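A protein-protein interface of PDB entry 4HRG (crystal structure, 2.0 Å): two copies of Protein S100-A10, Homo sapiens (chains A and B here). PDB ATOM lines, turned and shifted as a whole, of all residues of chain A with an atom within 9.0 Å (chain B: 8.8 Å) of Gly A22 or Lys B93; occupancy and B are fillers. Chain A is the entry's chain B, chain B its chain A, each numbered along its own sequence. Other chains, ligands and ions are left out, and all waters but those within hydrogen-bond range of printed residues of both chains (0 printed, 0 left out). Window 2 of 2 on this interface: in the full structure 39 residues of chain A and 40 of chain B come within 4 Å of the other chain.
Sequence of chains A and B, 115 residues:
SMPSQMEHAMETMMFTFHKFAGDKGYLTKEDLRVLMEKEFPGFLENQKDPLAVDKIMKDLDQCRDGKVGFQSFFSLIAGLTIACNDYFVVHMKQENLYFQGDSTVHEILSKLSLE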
ATOM      1  N   MET A  14      16.783  27.469  27.492  1.00  0.00           N
ATOM      2  CA  MET A  14      15.924  26.273  27.477  1.00  0.00           C
ATOM      3  C   MET A  14      15.356  25.960  26.117  1.00  0.00           C
ATOM      4  O   MET A  14      15.393  24.801  25.667  1.00  0.00           O
ATOM      5  CB  MET A  14      14.751  26.454  28.473  1.00  0.00           C
ATOM      6  CG  MET A  14      13.935  25.236  28.751  1.00  0.00           C
ATOM      7  SD  MET A  14      12.729  25.577  30.084  1.00  0.00           S
ATOM      8  CE  MET A  14      11.418  26.270  29.066  1.00  0.00           C
ATOM      9  N   PHE A  15      14.760  26.953  25.464  1.00  0.00           N
ATOM     10  CA  PHE A  15      14.128  26.686  24.181  1.00  0.00           C
ATOM     11  C   PHE A  15      15.121  26.496  23.045  1.00  0.00           C
ATOM     12  O   PHE A  15      14.819  25.835  22.051  1.00  0.00           O
ATOM     13  CB  PHE A  15      13.100  27.767  23.841  1.00  0.00           C
ATOM     14  CG  PHE A  15      11.857  27.718  24.706  1.00  0.00           C
ATOM     15  CD1 PHE A  15      10.963  26.666  24.600  1.00  0.00           C
ATOM     16  CD2 PHE A  15      11.585  28.732  25.618  1.00  0.00           C
ATOM     17  CE1 PHE A  15       9.826  26.633  25.389  1.00  0.00           C
ATOM     18  CE2 PHE A  15      10.454  28.708  26.396  1.00  0.00           C
ATOM     19  CZ  PHE A  15       9.583  27.662  26.295  1.00  0.00           C
ATOM     20  N   THR A  16      16.300  27.106  23.153  1.00  0.00           N
ATOM     21  CA  THR A  16      17.351  26.816  22.172  1.00  0.00           C
ATOM     22  C   THR A  16      17.748  25.344  22.229  1.00  0.00           C
ATOM     23  O   THR A  16      17.943  24.698  21.207  1.00  0.00           O
ATOM     24  CB  THR A  16      18.610  27.685  22.394  1.00  0.00           C
ATOM     25  OG1 THR A  16      18.226  29.068  22.309  1.00  0.00           O
ATOM     26  CG2 THR A  16      19.662  27.352  21.259  1.00  0.00           C
ATOM     27  N   PHE A  17      17.855  24.793  23.431  1.00  0.00           N
ATOM     28  CA  PHE A  17      18.246  23.393  23.531  1.00  0.00           C
ATOM     29  C   PHE A  17      17.208  22.523  22.859  1.00  0.00           C
ATOM     30  O   PHE A  17      17.533  21.645  22.031  1.00  0.00           O
ATOM     31  CB  PHE A  17      18.389  23.003  25.008  1.00  0.00           C
ATOM     32  CG  PHE A  17      18.546  21.510  25.227  1.00  0.00           C
ATOM     33  CD1 PHE A  17      19.786  20.908  25.087  1.00  0.00           C
ATOM     34  CD2 PHE A  17      17.454  20.726  25.591  1.00  0.00           C
ATOM     35  CE1 PHE A  17      19.948  19.557  25.306  1.00  0.00           C
ATOM     36  CE2 PHE A  17      17.602  19.357  25.796  1.00  0.00           C
ATOM     37  CZ  PHE A  17      18.850  18.768  25.647  1.00  0.00           C
ATOM     38  N   HIS A  18      15.939  22.740  23.212  1.00  0.00           N
ATOM     39  CA  HIS A  18      14.861  21.906  22.654  1.00  0.00           C
ATOM     40  C   HIS A  18      14.606  22.083  21.154  1.00  0.00           C
ATOM     41  O   HIS A  18      14.121  21.163  20.450  1.00  0.00           O
ATOM     42  CB  HIS A  18      13.572  22.107  23.462  1.00  0.00           C
ATOM     43  CG  HIS A  18      13.656  21.525  24.853  1.00  0.00           C
ATOM     44  ND1 HIS A  18      13.624  20.185  25.082  1.00  0.00           N
ATOM     45  CD2 HIS A  18      13.772  22.144  26.046  1.00  0.00           C
ATOM     46  CE1 HIS A  18      13.716  19.971  26.404  1.00  0.00           C
ATOM     47  NE2 HIS A  18      13.818  21.148  26.995  1.00  0.00           N
ATOM     48  N   LYS A  19      14.895  23.262  20.638  1.00  0.00           N
ATOM     49  CA  LYS A  19      14.756  23.471  19.210  1.00  0.00           C
ATOM     50  C   LYS A  19      15.717  22.529  18.504  1.00  0.00           C
ATOM     51  O   LYS A  19      15.359  21.921  17.490  1.00  0.00           O
ATOM     52  CB  LYS A  19      15.147  24.903  18.853  1.00  0.00           C
ATOM     53  CG  LYS A  19      14.789  25.324  17.423  1.00  0.00           C
ATOM     54  CD  LYS A  19      13.296  25.633  17.310  1.00  0.00           C
ATOM     55  CE  LYS A  19      12.841  25.760  15.861  1.00  0.00           C
ATOM     56  NZ  LYS A  19      11.354  25.834  15.765  1.00  0.00           N
ATOM     57  N   PHE A  20      16.943  22.408  19.015  1.00  0.00           N
ATOM     58  CA  PHE A  20      17.941  21.597  18.307  1.00  0.00           C
ATOM     59  C   PHE A  20      17.971  20.133  18.739  1.00  0.00           C
ATOM     60  O   PHE A  20      18.407  19.277  17.983  1.00  0.00           O
ATOM     61  CB  PHE A  20      19.328  22.235  18.402  1.00  0.00           C
ATOM     62  CG  PHE A  20      19.476  23.462  17.548  1.00  0.00           C
ATOM     63  CD1 PHE A  20      19.720  23.342  16.184  1.00  0.00           C
ATOM     64  CD2 PHE A  20      19.347  24.725  18.101  1.00  0.00           C
ATOM     65  CE1 PHE A  20      19.842  24.462  15.379  1.00  0.00           C
ATOM     66  CE2 PHE A  20      19.477  25.862  17.308  1.00  0.00           C
ATOM     67  CZ  PHE A  20      19.739  25.726  15.940  1.00  0.00           C
ATOM     68  N   ALA A  21      17.466  19.832  19.931  1.00  0.00           N
ATOM     69  CA  ALA A  21      17.454  18.456  20.401  1.00  0.00           C
ATOM     70  C   ALA A  21      16.243  17.681  19.862  1.00  0.00           C
ATOM     71  O   ALA A  21      16.275  16.455  19.790  1.00  0.00           O
ATOM     72  CB  ALA A  21      17.452  18.397  21.922  1.00  0.00           C
ATOM     73  N   GLY A  22      15.170  18.406  19.551  1.00  0.00           N
ATOM     74  CA  GLY A  22      13.912  17.818  19.113  1.00  0.00           C
ATOM     75  C   GLY A  22      13.277  16.869  20.106  1.00  0.00           C
ATOM     76  O   GLY A  22      13.601  16.872  21.294  1.00  0.00           O
ATOM     77  N   ASP A  23      12.366  16.046  19.591  1.00  0.00           N
ATOM     78  CA  ASP A  23      11.603  15.076  20.362  1.00  0.00           C
ATOM     79  C   ASP A  23      12.487  14.131  21.185  1.00  0.00           C
ATOM     80  O   ASP A  23      12.147  13.817  22.314  1.00  0.00           O
ATOM     81  CB  ASP A  23      10.697  14.278  19.414  1.00  0.00           C
ATOM     82  CG  ASP A  23       9.681  13.434  20.147  1.00  0.00           C
ATOM     83  OD1 ASP A  23      10.061  12.359  20.659  1.00  0.00           O
ATOM     84  OD2 ASP A  23       8.498  13.835  20.205  1.00  0.00           O
ATOM     85  N   LYS A  24      13.621  13.686  20.644  1.00  0.00           N
ATOM     86  CA  LYS A  24      14.470  12.746  21.382  1.00  0.00           C
ATOM     87  C   LYS A  24      14.998  13.382  22.678  1.00  0.00           C
ATOM     88  O   LYS A  24      15.352  12.684  23.645  1.00  0.00           O
ATOM     89  CB  LYS A  24      15.621  12.232  20.510  1.00  0.00           C
ATOM     90  CG  LYS A  24      16.785  13.245  20.287  1.00  0.00           C
ATOM     91  CD  LYS A  24      17.709  12.697  19.184  1.00  0.00           C
ATOM     92  CE  LYS A  24      18.793  13.685  18.803  1.00  0.00           C
ATOM     93  NZ  LYS A  24      18.225  14.984  18.351  1.00  0.00           N
ATOM     94  N   GLY A  25      15.045  14.712  22.715  1.00  0.00           N
ATOM     95  CA  GLY A  25      15.385  15.420  23.938  1.00  0.00           C
ATOM     96  C   GLY A  25      16.851  15.447  24.325  1.00  0.00           C
ATOM     97  O   GLY A  25      17.207  15.763  25.460  1.00  0.00           O
ATOM     98  N   TYR A  26      17.714  15.131  23.375  1.00  0.00           N
ATOM     99  CA  TYR A  26      19.147  15.335  23.568  1.00  0.00           C
ATOM    100  C   TYR A  26      19.769  15.788  22.256  1.00  0.00           C
ATOM    101  O   TYR A  26      19.146  15.665  21.187  1.00  0.00           O
ATOM    102  CB  TYR A  26      19.841  14.056  24.080  1.00  0.00           C
ATOM    103  CG  TYR A  26      19.722  12.882  23.144  1.00  0.00           C
ATOM    104  CD1 TYR A  26      20.645  12.698  22.124  1.00  0.00           C
ATOM    105  CD2 TYR A  26      18.697  11.952  23.285  1.00  0.00           C
ATOM    106  CE1 TYR A  26      20.556  11.632  21.257  1.00  0.00           C
ATOM    107  CE2 TYR A  26      18.599  10.852  22.413  1.00  0.00           C
ATOM    108  CZ  TYR A  26      19.528  10.711  21.413  1.00  0.00           C
ATOM    109  OH  TYR A  26      19.458   9.653  20.552  1.00  0.00           O
ATOM    110  N   LEU A  27      20.991  16.303  22.345  1.00  0.00           N
ATOM    111  CA  LEU A  27      21.762  16.729  21.169  1.00  0.00           C
ATOM    112  C   LEU A  27      22.775  15.667  20.777  1.00  0.00           C
ATOM    113  O   LEU A  27      23.457  15.117  21.643  1.00  0.00           O
ATOM    114  CB  LEU A  27      22.532  18.029  21.464  1.00  0.00           C
ATOM    115  CG  LEU A  27      21.719  19.268  21.796  1.00  0.00           C
ATOM    116  CD1 LEU A  27      22.611  20.446  22.333  1.00  0.00           C
ATOM    117  CD2 LEU A  27      20.917  19.683  20.578  1.00  0.00           C
ATOM    118  N   THR A  28      22.883  15.386  19.476  1.00  0.00           N
ATOM    119  CA  THR A  28      23.987  14.593  18.975  1.00  0.00           C
ATOM    120  C   THR A  28      25.171  15.519  18.783  1.00  0.00           C
ATOM    121  O   THR A  28      25.096  16.732  19.072  1.00  0.00           O
ATOM    122  CB  THR A  28      23.680  13.880  17.590  1.00  0.00           C
ATOM    123  OG1 THR A  28      23.473  14.866  16.574  1.00  0.00           O
ATOM    124  CG2 THR A  28      22.459  12.996  17.670  1.00  0.00           C
ATOM    125  N   ASP A  31      23.988  17.712  16.044  1.00  0.00           N
ATOM    126  CA  ASP A  31      23.011  18.698  16.495  1.00  0.00           C
ATOM    127  C   ASP A  31      23.737  19.842  17.175  1.00  0.00           C
ATOM    128  O   ASP A  31      23.398  21.022  16.989  1.00  0.00           O
ATOM    129  CB  ASP A  31      22.015  18.111  17.517  1.00  0.00           C
ATOM    130  CG  ASP A  31      21.092  17.081  16.934  1.00  0.00           C
ATOM    131  OD1 ASP A  31      20.794  17.127  15.710  1.00  0.00           O
ATOM    132  OD2 ASP A  31      20.656  16.209  17.720  1.00  0.00           O
ATOM    133  N   VAL A  68      24.156  14.725  24.359  1.00  0.00           N
ATOM    134  CA  VAL A  68      24.273  15.927  25.185  1.00  0.00           C
ATOM    135  C   VAL A  68      22.886  16.283  25.741  1.00  0.00           C
ATOM    136  O   VAL A  68      22.013  16.739  24.997  1.00  0.00           O
ATOM    137  CB  VAL A  68      24.861  17.120  24.393  1.00  0.00           C
ATOM    138  CG1 VAL A  68      25.126  18.340  25.313  1.00  0.00           C
ATOM    139  CG2 VAL A  68      26.164  16.730  23.711  1.00  0.00           C
ATOM    140  N   CYS B  84      13.851  24.463  36.040  1.00  0.00           N
ATOM    141  CA  CYS B  84      12.793  24.897  35.133  1.00  0.00           C
ATOM    142  C   CYS B  84      12.674  23.925  33.957  1.00  0.00           C
ATOM    143  O   CYS B  84      11.577  23.587  33.531  1.00  0.00           O
ATOM    144  CB  CYS B  84      13.064  26.279  34.543  1.00  0.00           C
ATOM    145  SG  CYS B  84      12.760  27.631  35.738  1.00  0.00           S
ATOM    146  N   ASN B  85      13.806  23.504  33.413  1.00  0.00           N
ATOM    147  CA  ASN B  85      13.750  22.632  32.247  1.00  0.00           C
ATOM    148  C   ASN B  85      13.094  21.317  32.603  1.00  0.00           C
ATOM    149  O   ASN B  85      12.294  20.761  31.836  1.00  0.00           O
ATOM    150  CB  ASN B  85      15.150  22.344  31.723  1.00  0.00           C
ATOM    151  CG  ASN B  85      15.126  21.518  30.485  1.00  0.00           C
ATOM    152  OD1 ASN B  85      14.584  21.953  29.453  1.00  0.00           O
ATOM    153  ND2 ASN B  85      15.718  20.302  30.555  1.00  0.00           N
ATOM    154  N   ASP B  86      13.456  20.777  33.754  1.00  0.00           N
ATOM    155  CA  ASP B  86      12.909  19.488  34.145  1.00  0.00           C
ATOM    156  C   ASP B  86      11.383  19.594  34.331  1.00  0.00           C
ATOM    157  O   ASP B  86      10.649  18.679  33.990  1.00  0.00           O
ATOM    158  CB  ASP B  86      13.546  19.038  35.468  1.00  0.00           C
ATOM    159  CG  ASP B  86      14.935  18.443  35.289  1.00  0.00           C
ATOM    160  OD1 ASP B  86      15.348  18.092  34.144  1.00  0.00           O
ATOM    161  OD2 ASP B  86      15.610  18.283  36.326  1.00  0.00           O
ATOM    162  N   TYR B  87      10.913  20.698  34.909  1.00  0.00           N
ATOM    163  CA  TYR B  87       9.476  20.925  35.043  1.00  0.00           C
ATOM    164  C   TYR B  87       8.806  20.988  33.672  1.00  0.00           C
ATOM    165  O   TYR B  87       7.741  20.397  33.442  1.00  0.00           O
ATOM    166  CB  TYR B  87       9.221  22.238  35.797  1.00  0.00           C
ATOM    167  CG  TYR B  87       7.761  22.510  36.034  1.00  0.00           C
ATOM    168  CD1 TYR B  87       6.972  23.079  35.049  1.00  0.00           C
ATOM    169  CD2 TYR B  87       7.156  22.165  37.249  1.00  0.00           C
ATOM    170  CE1 TYR B  87       5.587  23.298  35.253  1.00  0.00           C
ATOM    171  CE2 TYR B  87       5.791  22.397  37.474  1.00  0.00           C
ATOM    172  CZ  TYR B  87       5.015  22.960  36.463  1.00  0.00           C
ATOM    173  OH  TYR B  87       3.673  23.196  36.674  1.00  0.00           O
ATOM    174  N   PHE B  88       9.442  21.734  32.768  1.00  0.00           N
ATOM    175  CA  PHE B  88       8.951  21.936  31.419  1.00  0.00           C
ATOM    176  C   PHE B  88       8.834  20.600  30.728  1.00  0.00           C
ATOM    177  O   PHE B  88       7.798  20.287  30.101  1.00  0.00           O
ATOM    178  CB  PHE B  88       9.943  22.810  30.653  1.00  0.00           C
ATOM    179  CG  PHE B  88       9.605  22.955  29.209  1.00  0.00           C
ATOM    180  CD1 PHE B  88       8.524  23.743  28.819  1.00  0.00           C
ATOM    181  CD2 PHE B  88      10.357  22.296  28.235  1.00  0.00           C
ATOM    182  CE1 PHE B  88       8.199  23.878  27.460  1.00  0.00           C
ATOM    183  CE2 PHE B  88      10.045  22.424  26.883  1.00  0.00           C
ATOM    184  CZ  PHE B  88       8.966  23.222  26.491  1.00  0.00           C
ATOM    185  N   VAL B  89       9.881  19.778  30.850  1.00  0.00           N
ATOM    186  CA  VAL B  89       9.867  18.471  30.176  1.00  0.00           C
ATOM    187  C   VAL B  89       8.776  17.560  30.762  1.00  0.00           C
ATOM    188  O   VAL B  89       8.100  16.853  30.024  1.00  0.00           O
ATOM    189  CB  VAL B  89      11.215  17.755  30.286  1.00  0.00           C
ATOM    190  CG1 VAL B  89      11.069  16.252  29.887  1.00  0.00           C
ATOM    191  CG2 VAL B  89      12.271  18.444  29.421  1.00  0.00           C
ATOM    192  N   VAL B  90       8.605  17.574  32.085  1.00  0.00           N
ATOM    193  CA  VAL B  90       7.594  16.707  32.702  1.00  0.00           C
ATOM    194  C   VAL B  90       6.154  17.172  32.447  1.00  0.00           C
ATOM    195  O   VAL B  90       5.233  16.362  32.196  1.00  0.00           O
ATOM    196  CB  VAL B  90       7.824  16.593  34.245  1.00  0.00           C
ATOM    197  CG1 VAL B  90       6.684  15.810  34.904  1.00  0.00           C
ATOM    198  CG2 VAL B  90       9.170  15.936  34.560  1.00  0.00           C
ATOM    199  N   HIS B  91       5.941  18.475  32.535  1.00  0.00           N
ATOM    200  CA  HIS B  91       4.581  19.020  32.655  1.00  0.00           C
ATOM    201  C   HIS B  91       4.049  19.847  31.484  1.00  0.00           C
ATOM    202  O   HIS B  91       2.831  20.060  31.397  1.00  0.00           O
ATOM    203  CB  HIS B  91       4.499  19.899  33.902  1.00  0.00           C
ATOM    204  CG  HIS B  91       4.497  19.121  35.189  1.00  0.00           C
ATOM    205  ND1 HIS B  91       5.549  19.162  36.084  1.00  0.00           N
ATOM    206  CD2 HIS B  91       3.594  18.264  35.708  1.00  0.00           C
ATOM    207  CE1 HIS B  91       5.278  18.373  37.110  1.00  0.00           C
ATOM    208  NE2 HIS B  91       4.092  17.817  36.910  1.00  0.00           N
ATOM    209  N   MET B  92       4.934  20.324  30.606  1.00  0.00           N
ATOM    210  CA  MET B  92       4.540  21.308  29.605  1.00  0.00           C
ATOM    211  C   MET B  92       4.834  20.892  28.165  1.00  0.00           C
ATOM    212  O   MET B  92       4.001  21.087  27.286  1.00  0.00           O
ATOM    213  CB  MET B  92       5.220  22.654  29.901  1.00  0.00           C
ATOM    214  CG  MET B  92       4.707  23.320  31.190  1.00  0.00           C
ATOM    215  SD  MET B  92       5.635  24.830  31.569  1.00  0.00           S
ATOM    216  CE  MET B  92       4.546  26.059  30.851  1.00  0.00           C
ATOM    217  N   LYS B  93       6.004  20.296  27.939  1.00  0.00           N
ATOM    218  CA  LYS B  93       6.517  20.060  26.575  1.00  0.00           C
ATOM    219  C   LYS B  93       5.542  19.264  25.689  1.00  0.00           C
ATOM    220  O   LYS B  93       5.289  19.621  24.527  1.00  0.00           O
ATOM    221  CB  LYS B  93       7.873  19.342  26.636  1.00  0.00           C
ATOM    222  CG  LYS B  93       8.636  19.307  25.303  1.00  0.00           C
ATOM    223  CD  LYS B  93      10.015  18.644  25.433  1.00  0.00           C
ATOM    224  CE  LYS B  93      10.713  18.555  24.056  1.00  0.00           C
ATOM    225  NZ  LYS B  93      12.077  17.911  24.127  1.00  0.00           N
ATOM    226  N   GLN B  94       4.975  18.200  26.237  1.00  0.00           N
ATOM    227  CA  GLN B  94       4.104  17.328  25.441  1.00  0.00           C
ATOM    228  C   GLN B  94       2.762  17.975  25.156  1.00  0.00           C
ATOM    229  O   GLN B  94       1.962  17.466  24.351  1.00  0.00           O
ATOM    230  CB  GLN B  94       3.851  16.008  26.178  1.00  0.00           C
ATOM    231  CG  GLN B  94       5.103  15.214  26.475  1.00  0.00           C
ATOM    232  CD  GLN B  94       5.978  15.046  25.252  1.00  0.00           C
ATOM    233  OE1 GLN B  94       5.482  14.830  24.140  1.00  0.00           O
ATOM    234  NE2 GLN B  94       7.289  15.150  25.447  1.00  0.00           N
ATOM    235  N   GLU B  95       2.514  19.091  25.828  1.00  0.00           N
ATOM    236  CA  GLU B  95       1.155  19.609  25.945  1.00  0.00           C
ATOM    237  C   GLU B  95       0.911  20.802  25.023  1.00  0.00           C
ATOM    238  O   GLU B  95      -0.231  21.213  24.811  1.00  0.00           O
ATOM    239  CB  GLU B  95       0.896  20.009  27.396  1.00  0.00           C
ATOM    240  CG  GLU B  95       1.685  19.186  28.412  1.00  0.00           C
ATOM    241  CD  GLU B  95       0.895  18.023  28.974  1.00  0.00           C
ATOM    242  OE1 GLU B  95      -0.216  17.758  28.464  1.00  0.00           O
ATOM    243  OE2 GLU B  95       1.389  17.380  29.932  1.00  0.00           O
ATOM    244  N   ASN B  96       1.985  21.359  24.476  1.00  0.00           N
ATOM    245  CA  ASN B  96       1.841  22.491  23.560  1.00  0.00           C
ATOM    246  C   ASN B  96       3.004  22.675  22.588  1.00  0.00           C
ATOM    247  O   ASN B  96       4.160  22.369  22.921  1.00  0.00           O
ATOM    248  CB  ASN B  96       1.608  23.788  24.335  1.00  0.00           C
ATOM    249  CG  ASN B  96       0.655  24.735  23.616  1.00  0.00           C
ATOM    250  OD1 ASN B  96       0.837  25.060  22.432  1.00  0.00           O
ATOM    251  ND2 ASN B  96      -0.389  25.166  24.328  1.00  0.00           N
ATOM    252  N   LEU B  97       2.690  23.178  21.387  1.00  0.00           N
ATOM    253  CA  LEU B  97       3.716  23.384  20.341  1.00  0.00           C
ATOM    254  C   LEU B  97       4.246  24.771  20.440  1.00  0.00           C
ATOM    255  O   LEU B  97       5.294  25.102  19.866  1.00  0.00           O
ATOM    256  CB  LEU B  97       3.115  23.209  18.947  1.00  0.00           C
ATOM    257  CG  LEU B  97       3.052  21.812  18.367  1.00  0.00           C
ATOM    258  CD1 LEU B  97       3.669  21.946  17.018  1.00  0.00           C
ATOM    259  CD2 LEU B  97       3.954  20.901  19.236  1.00  0.00           C
ATOM    260  N   TYR B  98       3.488  25.607  21.131  1.00  0.00           N
ATOM    261  CA  TYR B  98       3.791  27.033  21.216  1.00  0.00           C
ATOM    262  C   TYR B  98       3.923  27.345  22.677  1.00  0.00           C
ATOM    263  O   TYR B  98       3.177  26.780  23.487  1.00  0.00           O
ATOM    264  CB  TYR B  98       2.598  27.858  20.676  1.00  0.00           C
ATOM    265  CG  TYR B  98       2.368  27.717  19.176  1.00  0.00           C
ATOM    266  CD1 TYR B  98       1.522  26.744  18.671  1.00  0.00           C
ATOM    267  CD2 TYR B  98       2.930  28.610  18.310  1.00  0.00           C
ATOM    268  CE1 TYR B  98       1.304  26.620  17.267  1.00  0.00           C
ATOM    269  CE2 TYR B  98       2.718  28.504  16.941  1.00  0.00           C
ATOM    270  CZ  TYR B  98       1.898  27.528  16.449  1.00  0.00           C
ATOM    271  OH  TYR B  98       1.736  27.465  15.078  1.00  0.00           O
ATOM    272  N   PHE B  99       4.858  28.227  23.030  1.00  0.00           N
ATOM    273  CA  PHE B  99       5.044  28.654  24.437  1.00  0.00           C
ATOM    274  C   PHE B  99       5.237  30.140  24.478  1.00  0.00           C
ATOM    275  O   PHE B  99       5.874  30.665  23.589  1.00  0.00           O
ATOM    276  CB  PHE B  99       6.245  27.903  25.075  1.00  0.00           C
ATOM    277  CG  PHE B  99       5.988  26.433  25.181  1.00  0.00           C
ATOM    278  CD1 PHE B  99       5.189  25.928  26.199  1.00  0.00           C
ATOM    279  CD2 PHE B  99       6.479  25.586  24.236  1.00  0.00           C
ATOM    280  CE1 PHE B  99       4.888  24.567  26.258  1.00  0.00           C
ATOM    281  CE2 PHE B  99       6.186  24.227  24.278  1.00  0.00           C
ATOM    282  CZ  PHE B  99       5.410  23.728  25.263  1.00  0.00           C
ATOM    283  N   ILE B 108       7.014  28.907  35.523  1.00  0.00           N
ATOM    284  CA  ILE B 108       7.677  27.757  36.129  1.00  0.00           C
ATOM    285  C   ILE B 108       8.418  28.097  37.418  1.00  0.00           C
ATOM    286  O   ILE B 108       8.469  27.290  38.329  1.00  0.00           O
ATOM    287  CB  ILE B 108       8.672  27.118  35.147  1.00  0.00           C
ATOM    288  CG1 ILE B 108       7.937  26.694  33.872  1.00  0.00           C
ATOM    289  CG2 ILE B 108       9.346  25.887  35.775  1.00  0.00           C
ATOM    290  CD1 ILE B 108       8.922  26.364  32.692  1.00  0.00           C
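The side-chain amide oxygen (OD1) of Asn B85 lies within hydrogen-bond range of a ring nitrogen (NE2) of His A18, at 2.7 Å.
A ring nitrogen (ND1) of His A18 sits at hydrogen-bond distance from the side-chain amino group (NZ) of Lys B93, at 2.9 Å.
NZ of Lys B93 is in hydrogen-bond range of O of Gly A22.
Among the printed residues, pairs that only touch across the chains: Met A14 with Asn B85 (3.4 Å), Phe A15 with Phe B99 (3.6 Å), His A18 with Val B89 (3.7 Å), Phe A15 with Phe B88 (3.7 Å), Met A14 with Phe B88 (3.8 Å) and His A18 with Phe B88 (3.8 Å).
N of Lys B93 sits at hydrogen-bond distance from O of Phe B88 (2.8 Å).
Gly A22 touches just one residue of chain B: Lys B93.
Of chain A, only His A18 (2.9 Å) and Gly A22 (3.4 Å) come within 4 Å of Lys B93.
No residue of chain A comes within 4 Å of Gln B94.
Printed residues of chain B within 4 Å of His A18: Asn B85 (2.7 Å), Phe B88 (3.8 Å), Val B89 (3.7 Å) and Lys B93 (2.9 Å).
Printed residues of chain A within 4 Å of Val B89: His A18.
Printed residues of chain A within 4 Å of Asn B85: Met A14 and His A18.
Of the printed residues of chain A, Phe B99 touches Phe A15 (3.6 Å).
Printed residues of chain A within 4 Å of Phe B88: Met A14 (3.8 Å), Phe A15 (3.7 Å) and His A18 (3.8 Å).
Met B92 touches none of the printed residues of chain A.
Ile B108 touches none of the printed residues of chain A.
Hydrophobic or aromatic side chains of chain B within 4 Å of the printed part of chain A: Phe B88, Val B89 and Phe B99.
Hydrophobic or aromatic side chains of chain A that line the printed part of chain B: Met A14, Phe A15 and His A18.
No position is printed for both chains.
Of the 9 pairs that touch across the chains among the printed residues, none has its exchanged pair printed and touching as well.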
